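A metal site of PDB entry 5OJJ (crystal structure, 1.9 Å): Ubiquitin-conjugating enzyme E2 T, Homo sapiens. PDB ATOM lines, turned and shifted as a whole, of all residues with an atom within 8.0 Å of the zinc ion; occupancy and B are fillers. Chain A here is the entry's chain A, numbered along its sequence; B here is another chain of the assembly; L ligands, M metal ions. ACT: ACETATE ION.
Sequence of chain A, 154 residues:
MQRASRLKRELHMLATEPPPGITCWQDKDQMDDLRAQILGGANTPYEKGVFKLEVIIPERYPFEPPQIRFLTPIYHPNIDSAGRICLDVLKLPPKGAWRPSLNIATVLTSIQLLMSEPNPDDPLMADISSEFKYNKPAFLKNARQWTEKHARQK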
ATOM      1  N   ASN A  78      -1.479  -3.378  -2.110  1.00  0.00           N
ATOM      2  CA  ASN A  78      -2.877  -3.745  -1.894  1.00  0.00           C
ATOM      3  C   ASN A  78      -3.697  -2.762  -1.042  1.00  0.00           C
ATOM      4  O   ASN A  78      -4.827  -3.073  -0.669  1.00  0.00           O
ATOM      5  CB  ASN A  78      -2.968  -5.150  -1.238  1.00  0.00           C
ATOM      6  CG  ASN A  78      -2.071  -6.192  -1.926  1.00  0.00           C
ATOM      7  OD1 ASN A  78      -1.286  -6.869  -1.262  1.00  0.00           O
ATOM      8  ND2 ASN A  78      -2.150  -6.279  -3.242  1.00  0.00           N
ATOM      9  N   ARG A  84      -8.246   1.935   1.529  1.00  0.00           N
ATOM     10  CA  ARG A  84      -9.003   0.756   1.153  1.00  0.00           C
ATOM     11  C   ARG A  84      -8.052  -0.418   0.979  1.00  0.00           C
ATOM     12  O   ARG A  84      -6.903  -0.216   0.557  1.00  0.00           O
ATOM     13  CB  ARG A  84      -9.789   0.967  -0.145  1.00  0.00           C
ATOM     14  CG  ARG A  84     -10.856   2.035  -0.040  1.00  0.00           C
ATOM     15  CD  ARG A  84     -11.626   2.249  -1.333  1.00  0.00           C
ATOM     16  NE  ARG A  84     -10.834   2.925  -2.370  1.00  0.00           N
ATOM     17  CZ  ARG A  84     -11.299   3.479  -3.489  1.00  0.00           C
ATOM     18  NH1 ARG A  84     -12.600   3.492  -3.762  1.00  0.00           N
ATOM     19  NH2 ARG A  84     -10.457   4.052  -4.328  1.00  0.00           N
ATOM     20  N   ILE A  85      -8.558  -1.623   1.263  1.00  0.00           N
ATOM     21  CA  ILE A  85      -7.714  -2.835   1.395  1.00  0.00           C
ATOM     22  C   ILE A  85      -8.226  -3.958   0.500  1.00  0.00           C
ATOM     23  O   ILE A  85      -9.380  -4.370   0.654  1.00  0.00           O
ATOM     24  CB  ILE A  85      -7.712  -3.357   2.859  1.00  0.00           C
ATOM     25  CG1 ILE A  85      -7.277  -2.278   3.854  1.00  0.00           C
ATOM     26  CG2 ILE A  85      -6.855  -4.632   2.980  1.00  0.00           C
ATOM     27  CD1 ILE A  85      -7.597  -2.586   5.292  1.00  0.00           C
ATOM     28  N   CYS A  86      -7.389  -4.462  -0.407  1.00  0.00           N
ATOM     29  CA  CYS A  86      -7.791  -5.599  -1.274  1.00  0.00           C
ATOM     30  C   CYS A  86      -7.391  -6.910  -0.605  1.00  0.00           C
ATOM     31  O   CYS A  86      -6.219  -7.273  -0.563  1.00  0.00           O
ATOM     32  CB  CYS A  86      -7.194  -5.514  -2.692  1.00  0.00           C
ATOM     33  SG  CYS A  86      -7.890  -6.744  -3.840  1.00  0.00           S
ATOM     34  N   LEU A  87      -8.398  -7.620  -0.068  1.00  0.00           N
ATOM     35  CA  LEU A  87      -8.161  -8.841   0.720  1.00  0.00           C
ATOM     36  C   LEU A  87      -9.367  -9.754   0.601  1.00  0.00           C
ATOM     37  O   LEU A  87     -10.502  -9.282   0.684  1.00  0.00           O
ATOM     38  CB  LEU A  87      -7.902  -8.459   2.184  1.00  0.00           C
ATOM     39  CG  LEU A  87      -7.548  -9.603   3.156  1.00  0.00           C
ATOM     40  CD1 LEU A  87      -6.295 -10.336   2.736  1.00  0.00           C
ATOM     41  CD2 LEU A  87      -7.400  -9.106   4.589  1.00  0.00           C
ATOM     42  N   ASP A  88      -9.127 -11.063   0.373  1.00  0.00           N
ATOM     43  CA  ASP A  88     -10.216 -12.030   0.110  1.00  0.00           C
ATOM     44  C   ASP A  88     -11.287 -12.079   1.193  1.00  0.00           C
ATOM     45  O   ASP A  88     -12.467 -12.093   0.870  1.00  0.00           O
ATOM     46  CB  ASP A  88      -9.696 -13.471  -0.174  1.00  0.00           C
ATOM     47  CG  ASP A  88      -8.854 -14.076   0.969  1.00  0.00           C
ATOM     48  OD1 ASP A  88      -8.551 -13.437   2.002  1.00  0.00           O
ATOM     49  OD2 ASP A  88      -8.464 -15.263   0.811  1.00  0.00           O
ATOM     50  N   LEU A  90     -12.420  -9.797   3.032  1.00  0.00           N
ATOM     51  CA  LEU A  90     -13.209  -8.596   3.007  1.00  0.00           C
ATOM     52  C   LEU A  90     -14.168  -8.516   1.827  1.00  0.00           C
ATOM     53  O   LEU A  90     -14.838  -7.482   1.649  1.00  0.00           O
ATOM     54  CB  LEU A  90     -12.298  -7.357   3.051  1.00  0.00           C
ATOM     55  CG  LEU A  90     -11.382  -7.249   4.279  1.00  0.00           C
ATOM     56  CD1 LEU A  90     -10.523  -5.988   4.194  1.00  0.00           C
ATOM     57  CD2 LEU A  90     -12.147  -7.265   5.609  1.00  0.00           C
ATOM     58  N   LYS A  91     -14.253  -9.606   1.037  1.00  0.00           N
ATOM     59  CA  LYS A  91     -15.092  -9.643  -0.160  1.00  0.00           C
ATOM     60  C   LYS A  91     -16.167 -10.737  -0.048  1.00  0.00           C
ATOM     61  O   LYS A  91     -15.941 -11.744   0.623  1.00  0.00           O
ATOM     62  CB  LYS A  91     -14.248  -9.864  -1.409  1.00  0.00           C
ATOM     63  CG  LYS A  91     -13.166  -8.812  -1.648  1.00  0.00           C
ATOM     64  CD  LYS A  91     -12.355  -9.175  -2.877  1.00  0.00           C
ATOM     65  CE  LYS A  91     -11.136  -8.306  -3.136  1.00  0.00           C
ATOM     66  NZ  LYS A  91     -11.592  -7.008  -3.650  1.00  0.00           N
ATOM     67  N   LYS A  95     -16.808 -15.174  -5.225  1.00  0.00           N
ATOM     68  CA  LYS A  95     -15.444 -14.696  -5.508  1.00  0.00           C
ATOM     69  C   LYS A  95     -14.620 -14.543  -4.217  1.00  0.00           C
ATOM     70  O   LYS A  95     -13.481 -14.990  -4.161  1.00  0.00           O
ATOM     71  CB  LYS A  95     -15.488 -13.383  -6.299  1.00  0.00           C
ATOM     72  CG  LYS A  95     -14.144 -12.700  -6.640  1.00  0.00           C
ATOM     73  CD  LYS A  95     -13.388 -12.182  -5.410  1.00  0.00           C
ATOM     74  CE  LYS A  95     -12.604 -10.909  -5.639  1.00  0.00           C
ATOM     75  NZ  LYS A  95     -11.294 -10.982  -6.308  1.00  0.00           N
ATOM     76  N   ASP A 122      -3.027  -8.309  -6.915  1.00  0.00           N
ATOM     77  CA  ASP A 122      -4.223  -7.623  -6.397  1.00  0.00           C
ATOM     78  C   ASP A 122      -3.992  -6.104  -6.228  1.00  0.00           C
ATOM     79  O   ASP A 122      -4.163  -5.573  -5.119  1.00  0.00           O
ATOM     80  CB  ASP A 122      -4.600  -8.215  -5.012  1.00  0.00           C
ATOM     81  CG  ASP A 122      -5.013  -9.680  -5.043  1.00  0.00           C
ATOM     82  OD1 ASP A 122      -5.259 -10.278  -6.123  1.00  0.00           O
ATOM     83  OD2 ASP A 122      -5.140 -10.231  -3.935  1.00  0.00           O
ATOM     84  N   PRO A 123      -3.653  -5.360  -7.307  1.00  0.00           N
ATOM     85  CA  PRO A 123      -3.246  -3.959  -7.077  1.00  0.00           C
ATOM     86  C   PRO A 123      -4.381  -2.966  -6.784  1.00  0.00           C
ATOM     87  O   PRO A 123      -5.415  -2.983  -7.463  1.00  0.00           O
ATOM     88  CB  PRO A 123      -2.571  -3.591  -8.406  1.00  0.00           C
ATOM     89  CG  PRO A 123      -3.314  -4.409  -9.421  1.00  0.00           C
ATOM     90  CD  PRO A 123      -3.573  -5.728  -8.736  1.00  0.00           C
ATOM     91  N   LEU A 124      -4.166  -2.099  -5.796  1.00  0.00           N
ATOM     92  CA  LEU A 124      -4.950  -0.853  -5.653  1.00  0.00           C
ATOM     93  C   LEU A 124      -4.136   0.430  -5.926  1.00  0.00           C
ATOM     94  O   LEU A 124      -4.727   1.507  -6.003  1.00  0.00           O
ATOM     95  CB  LEU A 124      -5.594  -0.765  -4.269  1.00  0.00           C
ATOM     96  CG  LEU A 124      -6.757  -1.722  -3.946  1.00  0.00           C
ATOM     97  CD1 LEU A 124      -7.221  -1.471  -2.517  1.00  0.00           C
ATOM     98  CD2 LEU A 124      -7.905  -1.563  -4.932  1.00  0.00           C
ATOM     99  N   THR B  72     -16.345   1.540  -4.365  1.00  0.00           N
ATOM    100  CA  THR B  72     -15.679   0.440  -5.102  1.00  0.00           C
ATOM    101  C   THR B  72     -14.522   1.018  -5.920  1.00  0.00           C
ATOM    102  O   THR B  72     -14.733   1.996  -6.629  1.00  0.00           O
ATOM    103  CB  THR B  72     -16.669  -0.204  -6.107  1.00  0.00           C
ATOM    104  OG1 THR B  72     -17.820  -0.678  -5.410  1.00  0.00           O
ATOM    105  CG2 THR B  72     -16.034  -1.342  -6.887  1.00  0.00           C
ATOM    106  N   PRO B  73     -13.306   0.427  -5.824  1.00  0.00           N
ATOM    107  CA  PRO B  73     -12.221   0.876  -6.702  1.00  0.00           C
ATOM    108  C   PRO B  73     -12.541   0.718  -8.181  1.00  0.00           C
ATOM    109  O   PRO B  73     -13.246  -0.206  -8.554  1.00  0.00           O
ATOM    110  CB  PRO B  73     -11.036  -0.051  -6.326  1.00  0.00           C
ATOM    111  CG  PRO B  73     -11.356  -0.591  -4.996  1.00  0.00           C
ATOM    112  CD  PRO B  73     -12.856  -0.619  -4.879  1.00  0.00           C
ATOM    113  N   TRP B 146      -8.901  -4.756 -13.167  1.00  0.00           N
ATOM    114  CA  TRP B 146      -9.404  -4.080 -11.953  1.00  0.00           C
ATOM    115  C   TRP B 146     -10.902  -4.350 -11.735  1.00  0.00           C
ATOM    116  O   TRP B 146     -11.359  -4.527 -10.606  1.00  0.00           O
ATOM    117  CB  TRP B 146      -9.114  -2.560 -11.966  1.00  0.00           C
ATOM    118  CG  TRP B 146      -7.697  -2.197 -11.595  1.00  0.00           C
ATOM    119  CD1 TRP B 146      -6.554  -2.720 -12.124  1.00  0.00           C
ATOM    120  CD2 TRP B 146      -7.269  -1.226 -10.627  1.00  0.00           C
ATOM    121  NE1 TRP B 146      -5.447  -2.162 -11.542  1.00  0.00           N
ATOM    122  CE2 TRP B 146      -5.854  -1.239 -10.617  1.00  0.00           C
ATOM    123  CE3 TRP B 146      -7.936  -0.346  -9.747  1.00  0.00           C
ATOM    124  CZ2 TRP B 146      -5.096  -0.397  -9.794  1.00  0.00           C
ATOM    125  CZ3 TRP B 146      -7.189   0.456  -8.930  1.00  0.00           C
ATOM    126  CH2 TRP B 146      -5.787   0.440  -8.960  1.00  0.00           C
ATOM    127  N   GLU B 148     -12.532  -7.132 -12.721  1.00  0.00           N
ATOM    128  CA  GLU B 148     -12.531  -8.520 -12.247  1.00  0.00           C
ATOM    129  C   GLU B 148     -12.121  -8.623 -10.779  1.00  0.00           C
ATOM    130  O   GLU B 148     -12.765  -9.319  -9.992  1.00  0.00           O
ATOM    131  CB  GLU B 148     -11.601  -9.378 -13.124  1.00  0.00           C
ATOM    132  CG  GLU B 148     -11.768 -10.889 -12.970  1.00  0.00           C
ATOM    133  CD  GLU B 148     -11.074 -11.489 -11.739  1.00  0.00           C
ATOM    134  OE1 GLU B 148      -9.895 -11.156 -11.475  1.00  0.00           O
ATOM    135  OE2 GLU B 148     -11.712 -12.308 -11.033  1.00  0.00           O
ATOM    136  N   LYS B 149     -11.055  -7.909 -10.405  1.00  0.00           N
ATOM    137  CA  LYS B 149     -10.508  -7.999  -9.038  1.00  0.00           C
ATOM    138  C   LYS B 149     -11.385  -7.382  -7.947  1.00  0.00           C
ATOM    139  O   LYS B 149     -11.611  -8.015  -6.898  1.00  0.00           O
ATOM    140  CB  LYS B 149      -9.115  -7.383  -8.992  1.00  0.00           C
ATOM    141  CG  LYS B 149      -8.331  -7.638  -7.705  1.00  0.00           C
ATOM    142  CD  LYS B 149      -8.092  -9.106  -7.425  1.00  0.00           C
ATOM    143  CE  LYS B 149      -7.462  -9.781  -8.637  1.00  0.00           C
ATOM    144  NZ  LYS B 149      -6.782 -11.032  -8.253  1.00  0.00           N
ATOM    145  N   HIS B 150     -11.876  -6.168  -8.188  1.00  0.00           N
ATOM    146  CA  HIS B 150     -12.502  -5.328  -7.156  1.00  0.00           C
ATOM    147  C   HIS B 150     -14.023  -5.120  -7.258  1.00  0.00           C
ATOM    148  O   HIS B 150     -14.656  -4.749  -6.273  1.00  0.00           O
ATOM    149  CB  HIS B 150     -11.845  -3.945  -7.153  1.00  0.00           C
ATOM    150  CG  HIS B 150     -10.360  -4.004  -7.175  1.00  0.00           C
ATOM    151  ND1 HIS B 150      -9.629  -4.732  -6.253  1.00  0.00           N
ATOM    152  CD2 HIS B 150      -9.452  -3.421  -7.995  1.00  0.00           C
ATOM    153  CE1 HIS B 150      -8.343  -4.599  -6.507  1.00  0.00           C
ATOM    154  NE2 HIS B 150      -8.206  -3.807  -7.564  1.00  0.00           N
ATOM    155  N   ALA B 151     -14.588  -5.300  -8.445  1.00  0.00           N
ATOM    156  CA  ALA B 151     -16.019  -5.112  -8.636  1.00  0.00           C
ATOM    157  C   ALA B 151     -16.658  -6.496  -8.827  1.00  0.00           C
ATOM    158  O   ALA B 151     -17.290  -7.013  -7.907  1.00  0.00           O
ATOM    159  CB  ALA B 151     -16.291  -4.192  -9.817  1.00  0.00           C
HETATM  160  C   ACT L   1     -11.194  -3.587  -2.851  1.00  0.00           C
HETATM  161  O   ACT L   1     -10.096  -4.138  -3.019  1.00  0.00           O
HETATM  162  OXT ACT L   1     -12.169  -3.927  -3.543  1.00  0.00           O
HETATM  163  CH3 ACT L   1     -11.347  -2.497  -1.822  1.00  0.00           C
HETATM  164 ZN    ZN M   1      -9.928  -5.710  -4.266  1.00  0.00          ZN
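OD1 of Asp 122 lies within salt-bridge range of NZ of Lys 149 of chain B. The backbone carbonyl oxygen of Lys 149 of chain B is in hydrogen-bond range of the side-chain amino group of Lys 95. NZ of Lys 91 sits close to O of Lys 149 of chain B (3.4 Å). O of Asn 78 is in hydrogen-bond range of N of Cys 86, at 2.9 Å. A ring nitrogen (NE2) of His 150 of chain B lies within hydrogen-bond range of the backbone carbonyl oxygen of Pro 123, at 2.9 Å.
O of Lys 149 of chain B touches the zinc ion, at 3.9 Å. The nearest printed residue that does not touch the zinc ion is Leu 124 (4.7 Å).
The zinc ion is bound by an oxygen (O) of the ligand (2.0 Å), the side-chain amino group (NZ) of Lys 91 (2.2 Å), a ring nitrogen (ND1) of His 150 of chain B (2.2 Å) and the side-chain sulfur (SG) of Cys 86 (2.3 Å).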
